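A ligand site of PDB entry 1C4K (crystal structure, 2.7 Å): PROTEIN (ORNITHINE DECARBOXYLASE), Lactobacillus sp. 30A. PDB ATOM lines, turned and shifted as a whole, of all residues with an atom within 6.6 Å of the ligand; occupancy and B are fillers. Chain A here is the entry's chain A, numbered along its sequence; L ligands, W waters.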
ATOM      1  N   GLY A 196       2.208  -9.763   9.313  1.00  0.00           N
ATOM      2  CA  GLY A 196       2.288  -9.940   7.876  1.00  0.00           C
ATOM      3  C   GLY A 196       2.221 -11.415   7.526  1.00  0.00           C
ATOM      4  O   GLY A 196       2.912 -11.863   6.624  1.00  0.00           O
ATOM      5  N   GLY A 197       1.433 -12.171   8.294  1.00  0.00           N
ATOM      6  CA  GLY A 197       1.292 -13.594   8.065  1.00  0.00           C
ATOM      7  C   GLY A 197       2.559 -14.381   8.230  1.00  0.00           C
ATOM      8  O   GLY A 197       3.609 -13.796   8.507  1.00  0.00           O
ATOM      9  N   SER A 198       2.463 -15.709   8.139  1.00  0.00           N
ATOM     10  CA  SER A 198       3.630 -16.577   8.274  1.00  0.00           C
ATOM     11  C   SER A 198       4.591 -16.415   7.101  1.00  0.00           C
ATOM     12  O   SER A 198       5.669 -16.983   7.125  1.00  0.00           O
ATOM     13  CB  SER A 198       3.253 -18.037   8.451  1.00  0.00           C
ATOM     14  OG  SER A 198       2.751 -18.231   9.735  1.00  0.00           O
ATOM     15  N   SER A 199       4.191 -15.608   6.119  1.00  0.00           N
ATOM     16  CA  SER A 199       5.000 -15.349   4.944  1.00  0.00           C
ATOM     17  C   SER A 199       6.132 -14.445   5.338  1.00  0.00           C
ATOM     18  O   SER A 199       7.274 -14.714   5.059  1.00  0.00           O
ATOM     19  CB  SER A 199       4.157 -14.709   3.854  1.00  0.00           C
ATOM     20  OG  SER A 199       3.049 -15.544   3.572  1.00  0.00           O
ATOM     21  N   ASN A 200       5.776 -13.394   6.056  1.00  0.00           N
ATOM     22  CA  ASN A 200       6.745 -12.418   6.530  1.00  0.00           C
ATOM     23  C   ASN A 200       7.457 -12.934   7.780  1.00  0.00           C
ATOM     24  O   ASN A 200       8.560 -12.515   8.061  1.00  0.00           O
ATOM     25  CB  ASN A 200       6.109 -11.051   6.721  1.00  0.00           C
ATOM     26  CG  ASN A 200       5.854 -10.393   5.410  1.00  0.00           C
ATOM     27  OD1 ASN A 200       6.793 -10.001   4.709  1.00  0.00           O
ATOM     28  ND2 ASN A 200       4.599 -10.358   5.011  1.00  0.00           N
ATOM     29  N   ASN A 202       8.283 -15.966   7.995  1.00  0.00           N
ATOM     30  CA  ASN A 202       9.207 -16.915   7.383  1.00  0.00           C
ATOM     31  C   ASN A 202      10.385 -16.103   6.875  1.00  0.00           C
ATOM     32  O   ASN A 202      11.506 -16.572   6.858  1.00  0.00           O
ATOM     33  CB  ASN A 202       8.578 -17.751   6.278  1.00  0.00           C
ATOM     34  CG  ASN A 202       8.035 -19.122   6.766  1.00  0.00           C
ATOM     35  OD1 ASN A 202       7.174 -19.736   6.094  1.00  0.00           O
ATOM     36  ND2 ASN A 202       8.537 -19.603   7.889  1.00  0.00           N
ATOM     37  N   ASN A 221       8.556 -30.073   0.521  1.00  0.00           N
ATOM     38  CA  ASN A 221       7.152 -29.675   0.722  1.00  0.00           C
ATOM     39  C   ASN A 221       6.992 -28.217   1.172  1.00  0.00           C
ATOM     40  O   ASN A 221       5.906 -27.678   1.144  1.00  0.00           O
ATOM     41  CB  ASN A 221       6.500 -30.541   1.797  1.00  0.00           C
ATOM     42  CG  ASN A 221       6.026 -31.869   1.269  1.00  0.00           C
ATOM     43  OD1 ASN A 221       5.675 -31.992   0.097  1.00  0.00           O
ATOM     44  ND2 ASN A 221       5.967 -32.849   2.144  1.00  0.00           N
ATOM     45  N   ASN A 222       8.096 -27.565   1.497  1.00  0.00           N
ATOM     46  CA  ASN A 222       8.061 -26.208   1.941  1.00  0.00           C
ATOM     47  C   ASN A 222       7.340 -25.211   1.090  1.00  0.00           C
ATOM     48  O   ASN A 222       7.503 -25.187  -0.113  1.00  0.00           O
ATOM     49  CB  ASN A 222       9.464 -25.703   2.234  1.00  0.00           C
ATOM     50  CG  ASN A 222       9.968 -26.158   3.568  1.00  0.00           C
ATOM     51  OD1 ASN A 222      11.170 -26.338   3.749  1.00  0.00           O
ATOM     52  ND2 ASN A 222       9.054 -26.378   4.511  1.00  0.00           N
ATOM     53  N   HIS A 223       6.600 -24.342   1.779  1.00  0.00           N
ATOM     54  CA  HIS A 223       5.783 -23.259   1.205  1.00  0.00           C
ATOM     55  C   HIS A 223       6.642 -22.295   0.372  1.00  0.00           C
ATOM     56  O   HIS A 223       7.854 -22.182   0.621  1.00  0.00           O
ATOM     57  CB  HIS A 223       5.094 -22.536   2.366  1.00  0.00           C
ATOM     58  CG  HIS A 223       4.014 -21.584   1.988  1.00  0.00           C
ATOM     59  ND1 HIS A 223       4.233 -20.227   1.849  1.00  0.00           N
ATOM     60  CD2 HIS A 223       2.677 -21.763   1.841  1.00  0.00           C
ATOM     61  CE1 HIS A 223       3.069 -19.617   1.644  1.00  0.00           C
ATOM     62  NE2 HIS A 223       2.119 -20.528   1.639  1.00  0.00           N
ATOM     63  N   LYS A 224       6.044 -21.593  -0.588  1.00  0.00           N
ATOM     64  CA  LYS A 224       6.780 -20.659  -1.443  1.00  0.00           C
ATOM     65  C   LYS A 224       7.615 -19.630  -0.691  1.00  0.00           C
ATOM     66  O   LYS A 224       8.743 -19.321  -1.114  1.00  0.00           O
ATOM     67  CB  LYS A 224       5.842 -19.989  -2.450  1.00  0.00           C
ATOM     68  CG  LYS A 224       4.684 -19.242  -1.831  1.00  0.00           C
ATOM     69  CD  LYS A 224       3.910 -18.399  -2.844  1.00  0.00           C
ATOM     70  CE  LYS A 224       3.400 -17.113  -2.155  1.00  0.00           C
ATOM     71  NZ  LYS A 224       2.538 -16.179  -2.962  1.00  0.00           N
ATOM     72  N   SER A 225       7.121 -19.166   0.455  1.00  0.00           N
ATOM     73  CA  SER A 225       7.815 -18.171   1.285  1.00  0.00           C
ATOM     74  C   SER A 225       9.139 -18.673   1.825  1.00  0.00           C
ATOM     75  O   SER A 225      10.034 -17.891   2.095  1.00  0.00           O
ATOM     76  CB  SER A 225       6.932 -17.715   2.457  1.00  0.00           C
ATOM     77  OG  SER A 225       6.622 -18.771   3.365  1.00  0.00           O
ATOM     78  N   VAL A 226       9.255 -19.985   2.006  1.00  0.00           N
ATOM     79  CA  VAL A 226      10.472 -20.563   2.517  1.00  0.00           C
ATOM     80  C   VAL A 226      11.470 -20.766   1.395  1.00  0.00           C
ATOM     81  O   VAL A 226      12.663 -20.934   1.649  1.00  0.00           O
ATOM     82  CB  VAL A 226      10.216 -21.848   3.275  1.00  0.00           C
ATOM     83  CG1 VAL A 226      11.474 -22.351   3.900  1.00  0.00           C
ATOM     84  CG2 VAL A 226       9.187 -21.632   4.357  1.00  0.00           C
ATOM     85  N   GLN A 288       8.271 -28.750   7.385  1.00  0.00           N
ATOM     86  CA  GLN A 288       6.879 -28.304   7.465  1.00  0.00           C
ATOM     87  C   GLN A 288       6.189 -29.304   8.396  1.00  0.00           C
ATOM     88  O   GLN A 288       5.769 -30.366   7.954  1.00  0.00           O
ATOM     89  CB  GLN A 288       6.283 -28.358   6.077  1.00  0.00           C
ATOM     90  CG  GLN A 288       4.897 -27.769   5.922  1.00  0.00           C
ATOM     91  CD  GLN A 288       4.292 -28.042   4.549  1.00  0.00           C
ATOM     92  OE1 GLN A 288       4.574 -29.072   3.933  1.00  0.00           O
ATOM     93  NE2 GLN A 288       3.457 -27.151   4.080  1.00  0.00           N
ATOM     94  N   GLY A 290       3.180 -29.581   9.798  1.00  0.00           N
ATOM     95  CA  GLY A 290       1.864 -30.046   9.462  1.00  0.00           C
ATOM     96  C   GLY A 290       1.538 -29.743   8.036  1.00  0.00           C
ATOM     97  O   GLY A 290       1.463 -28.584   7.631  1.00  0.00           O
ATOM     98  N   ASP A 316       7.814 -25.094  10.262  1.00  0.00           N
ATOM     99  CA  ASP A 316       6.772 -24.233   9.677  1.00  0.00           C
ATOM    100  C   ASP A 316       5.508 -24.970  10.123  1.00  0.00           C
ATOM    101  O   ASP A 316       5.147 -26.002   9.558  1.00  0.00           O
ATOM    102  CB  ASP A 316       6.863 -24.177   8.140  1.00  0.00           C
ATOM    103  CG  ASP A 316       6.014 -23.066   7.541  1.00  0.00           C
ATOM    104  OD1 ASP A 316       5.021 -22.622   8.173  1.00  0.00           O
ATOM    105  OD2 ASP A 316       6.332 -22.603   6.425  1.00  0.00           O
ATOM    106  N   SER A 317       4.929 -24.496  11.218  1.00  0.00           N
ATOM    107  CA  SER A 317       3.723 -25.071  11.820  1.00  0.00           C
ATOM    108  C   SER A 317       2.462 -24.260  11.537  1.00  0.00           C
ATOM    109  O   SER A 317       1.510 -24.273  12.319  1.00  0.00           O
ATOM    110  CB  SER A 317       3.937 -25.198  13.329  1.00  0.00           C
ATOM    111  OG  SER A 317       5.139 -25.900  13.591  1.00  0.00           O
ATOM    112  N   ALA A 318       2.479 -23.545  10.419  1.00  0.00           N
ATOM    113  CA  ALA A 318       1.343 -22.716  10.013  1.00  0.00           C
ATOM    114  C   ALA A 318       0.011 -23.448   9.850  1.00  0.00           C
ATOM    115  O   ALA A 318      -1.043 -22.828   9.936  1.00  0.00           O
ATOM    116  CB  ALA A 318       1.685 -21.979   8.755  1.00  0.00           C
ATOM    117  N   TRP A 319       0.058 -24.739   9.539  1.00  0.00           N
ATOM    118  CA  TRP A 319      -1.169 -25.496   9.374  1.00  0.00           C
ATOM    119  C   TRP A 319      -1.588 -26.189  10.659  1.00  0.00           C
ATOM    120  O   TRP A 319      -2.608 -26.893  10.686  1.00  0.00           O
ATOM    121  CB  TRP A 319      -1.112 -26.508   8.233  1.00  0.00           C
ATOM    122  CG  TRP A 319      -1.524 -25.947   6.918  1.00  0.00           C
ATOM    123  CD1 TRP A 319      -0.795 -25.921   5.790  1.00  0.00           C
ATOM    124  CD2 TRP A 319      -2.775 -25.273   6.621  1.00  0.00           C
ATOM    125  NE1 TRP A 319      -1.492 -25.264   4.793  1.00  0.00           N
ATOM    126  CE2 TRP A 319      -2.716 -24.862   5.277  1.00  0.00           C
ATOM    127  CE3 TRP A 319      -3.940 -24.994   7.359  1.00  0.00           C
ATOM    128  CZ2 TRP A 319      -3.769 -24.164   4.652  1.00  0.00           C
ATOM    129  CZ3 TRP A 319      -4.994 -24.296   6.734  1.00  0.00           C
ATOM    130  CH2 TRP A 319      -4.894 -23.897   5.388  1.00  0.00           C
ATOM    131  N   VAL A 350       7.249 -21.322  13.706  1.00  0.00           N
ATOM    132  CA  VAL A 350       6.431 -20.313  13.049  1.00  0.00           C
ATOM    133  C   VAL A 350       5.005 -20.848  12.872  1.00  0.00           C
ATOM    134  O   VAL A 350       4.866 -21.967  12.420  1.00  0.00           O
ATOM    135  CB  VAL A 350       6.976 -19.959  11.640  1.00  0.00           C
ATOM    136  CG1 VAL A 350       6.065 -18.956  10.958  1.00  0.00           C
ATOM    137  CG2 VAL A 350       8.396 -19.353  11.742  1.00  0.00           C
ATOM    138  N   GLN A 351       3.982 -20.110  13.277  1.00  0.00           N
ATOM    139  CA  GLN A 351       2.612 -20.629  13.176  1.00  0.00           C
ATOM    140  C   GLN A 351       1.665 -19.549  12.821  1.00  0.00           C
ATOM    141  O   GLN A 351       1.796 -18.429  13.301  1.00  0.00           O
ATOM    142  CB  GLN A 351       2.152 -21.342  14.443  1.00  0.00           C
ATOM    143  CG  GLN A 351       2.317 -20.546  15.668  1.00  0.00           C
ATOM    144  CD  GLN A 351       1.865 -21.310  16.885  1.00  0.00           C
ATOM    145  OE1 GLN A 351       1.230 -20.749  17.771  1.00  0.00           O
ATOM    146  NE2 GLN A 351       2.346 -22.559  17.032  1.00  0.00           N
ATOM    147  N   SER A 352       0.777 -19.785  11.835  1.00  0.00           N
ATOM    148  CA  SER A 352      -0.208 -18.811  11.383  1.00  0.00           C
ATOM    149  C   SER A 352      -1.378 -18.986  12.293  1.00  0.00           C
ATOM    150  O   SER A 352      -2.098 -19.965  12.095  1.00  0.00           O
ATOM    151  CB  SER A 352      -0.678 -19.101   9.989  1.00  0.00           C
ATOM    152  OG  SER A 352       0.276 -18.799   8.967  1.00  0.00           O
ATOM    153  N   VAL A 353      -1.596 -18.026  13.193  1.00  0.00           N
ATOM    154  CA  VAL A 353      -2.686 -18.046  14.150  1.00  0.00           C
ATOM    155  C   VAL A 353      -4.068 -18.051  13.499  1.00  0.00           C
ATOM    156  O   VAL A 353      -4.961 -18.747  14.009  1.00  0.00           O
ATOM    157  CB  VAL A 353      -2.518 -16.901  15.201  1.00  0.00           C
ATOM    158  CG1 VAL A 353      -3.784 -16.670  16.030  1.00  0.00           C
ATOM    159  CG2 VAL A 353      -1.372 -17.223  16.132  1.00  0.00           C
ATOM    160  N   HIS A 354      -4.216 -17.389  12.370  1.00  0.00           N
ATOM    161  CA  HIS A 354      -5.492 -17.304  11.614  1.00  0.00           C
ATOM    162  C   HIS A 354      -5.959 -18.588  10.958  1.00  0.00           C
ATOM    163  O   HIS A 354      -7.161 -18.754  10.822  1.00  0.00           O
ATOM    164  CB  HIS A 354      -5.428 -16.222  10.541  1.00  0.00           C
ATOM    165  CG  HIS A 354      -4.424 -16.489   9.451  1.00  0.00           C
ATOM    166  ND1 HIS A 354      -3.194 -15.908   9.438  1.00  0.00           N
ATOM    167  CD2 HIS A 354      -4.510 -17.169   8.296  1.00  0.00           C
ATOM    168  CE1 HIS A 354      -2.553 -16.192   8.317  1.00  0.00           C
ATOM    169  NE2 HIS A 354      -3.335 -16.965   7.606  1.00  0.00           N
ATOM    170  N   LYS A 355      -5.026 -19.416  10.536  1.00  0.00           N
ATOM    171  CA  LYS A 355      -5.427 -20.676   9.870  1.00  0.00           C
ATOM    172  C   LYS A 355      -6.305 -21.584  10.719  1.00  0.00           C
ATOM    173  O   LYS A 355      -7.491 -21.691  10.429  1.00  0.00           O
ATOM    174  CB  LYS A 355      -4.236 -21.392   9.228  1.00  0.00           C
ATOM    175  CG  LYS A 355      -3.791 -20.648   7.951  1.00  0.00           C
ATOM    176  CD  LYS A 355      -2.635 -21.325   7.293  1.00  0.00           C
ATOM    177  CE  LYS A 355      -2.372 -20.734   5.931  1.00  0.00           C
ATOM    178  NZ  LYS A 355      -1.059 -21.068   5.854  1.00  0.00           N
ATOM    179  N   GLN A 362      -3.737 -12.653   8.411  1.00  0.00           N
ATOM    180  CA  GLN A 362      -2.428 -11.998   8.404  1.00  0.00           C
ATOM    181  C   GLN A 362      -1.756 -12.007   9.776  1.00  0.00           C
ATOM    182  O   GLN A 362      -0.692 -11.423   9.947  1.00  0.00           O
ATOM    183  CB  GLN A 362      -2.496 -10.563   7.915  1.00  0.00           C
ATOM    184  CG  GLN A 362      -1.897 -10.297   6.579  1.00  0.00           C
ATOM    185  CD  GLN A 362      -1.982  -8.834   6.208  1.00  0.00           C
ATOM    186  OE1 GLN A 362      -1.370  -7.975   6.843  1.00  0.00           O
ATOM    187  NE2 GLN A 362      -2.748  -8.553   5.157  1.00  0.00           N
ATOM    188  N   THR A 363      -2.369 -12.639  10.774  1.00  0.00           N
ATOM    189  CA  THR A 363      -1.741 -12.668  12.092  1.00  0.00           C
ATOM    190  C   THR A 363      -0.979 -13.960  12.260  1.00  0.00           C
ATOM    191  O   THR A 363      -1.496 -15.036  11.950  1.00  0.00           O
ATOM    192  CB  THR A 363      -2.739 -12.608  13.271  1.00  0.00           C
ATOM    193  OG1 THR A 363      -3.675 -13.676  13.184  1.00  0.00           O
ATOM    194  CG2 THR A 363      -3.425 -11.261  13.336  1.00  0.00           C
ATOM    195  N   SER A 364       0.248 -13.858  12.758  1.00  0.00           N
ATOM    196  CA  SER A 364       1.061 -15.036  12.973  1.00  0.00           C
ATOM    197  C   SER A 364       2.046 -14.737  14.100  1.00  0.00           C
ATOM    198  O   SER A 364       2.087 -13.608  14.609  1.00  0.00           O
ATOM    199  CB  SER A 364       1.786 -15.489  11.691  1.00  0.00           C
ATOM    200  OG  SER A 364       3.028 -14.866  11.484  1.00  0.00           O
HETATM  201  N1  LIG L   1       3.933 -21.823   5.522  1.00  0.00           N
HETATM  202  C1  LIG L   1       2.896 -22.767   5.517  1.00  0.00           C
HETATM  203  C2  LIG L   1       3.168 -24.235   5.669  1.00  0.00           C
HETATM  204  C3  LIG L   1       1.588 -22.355   5.321  1.00  0.00           C
HETATM  205  C4  LIG L   1       1.290 -21.014   5.091  1.00  0.00           C
HETATM  206  C5  LIG L   1      -0.234 -20.565   4.947  1.00  0.00           C
HETATM  207  C6  LIG L   1       2.335 -20.089   5.064  1.00  0.00           C
HETATM  208  C7  LIG L   1       3.654 -20.490   5.298  1.00  0.00           C
HETATM  209  C8  LIG L   1       2.042 -18.609   4.728  1.00  0.00           C
HETATM  210  O1  LIG L   1       1.385 -18.093   5.864  1.00  0.00           O
HETATM  211  P1  LIG L   1       0.470 -16.928   5.709  1.00  0.00           P
HETATM  212  O2  LIG L   1      -0.699 -17.556   5.164  1.00  0.00           O
HETATM  213  O3  LIG L   1       0.772 -15.664   5.077  1.00  0.00           O
HETATM  214  O4  LIG L   1       0.158 -16.690   7.116  1.00  0.00           O
HETATM  215  O   HOH W   1       6.429 -24.756   4.804  1.00  0.00           O
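Water W1 lies within hydrogen-bond range of OD2 of Asp 316 (2.7 Å), N of His 223 (3.1 Å) and ND2 of Asn 222 (3.1 Å).
A nitrogen (N1) of the ligand lies within hydrogen-bond range of the side-chain carboxylate (OD2) of Asp 316 (2.7 Å). NZ of Lys 355 is bonded to C5 of the ligand (1.3 Å). An oxygen (O4) of the ligand lies within hydrogen-bond range of the side-chain hydroxyl of Ser 352 (2.8 Å). An oxygen (O3) of the ligand is in hydrogen-bond range of the side-chain hydroxyl (OG) of Ser 199 (2.7 Å). An oxygen (O4) of the ligand lies within hydrogen-bond range of the backbone NH of Ser 198 (2.7 Å).
The backbone carbonyl oxygen (O) of Asn 221 sits close to the side-chain amide oxygen (OE1) of Gln 288 (3.4 Å). The side-chain hydroxyl (OG) of Ser 352 lies within hydrogen-bond range of the side-chain hydroxyl (OG) of Ser 198, at 2.7 Å. The side-chain hydroxyl (OG) of Ser 225 is in hydrogen-bond range of a ring nitrogen (ND1) of His 223, at 3.2 Å. OD1 of Asn 202 is in hydrogen-bond range of OG of Ser 225, at 2.9 Å. The backbone NH (N) of Gly 197 is in hydrogen-bond range of the backbone carbonyl oxygen (O) of Gln 362. The side-chain amide oxygen (OD1) of Asn 202 sits close to the side-chain carboxylate (OD2) of Asp 316. N of Ala 318 is in hydrogen-bond range of O of Val 350 (3.5 Å). O of Thr 363 sits at hydrogen-bond distance from ND1 of His 354.
Merely in contact with the ligand: His 354, Gln 288, His 223, Gly 197, Ala 318, Asn 202 and Ser 225. Hydrophobic or aromatic side chains that line the ligand: His 223, Ala 318 and His 354. Within 4 Å of the ligand: Gly 197, Ser 198, Ser 199, Asn 202, His 223, Ser 225, Gln 288, Asp 316, Ala 318, Ser 352, His 354 and Lys 355. The nearest printed residue that does not touch the ligand is Trp 319 (4.3 Å).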
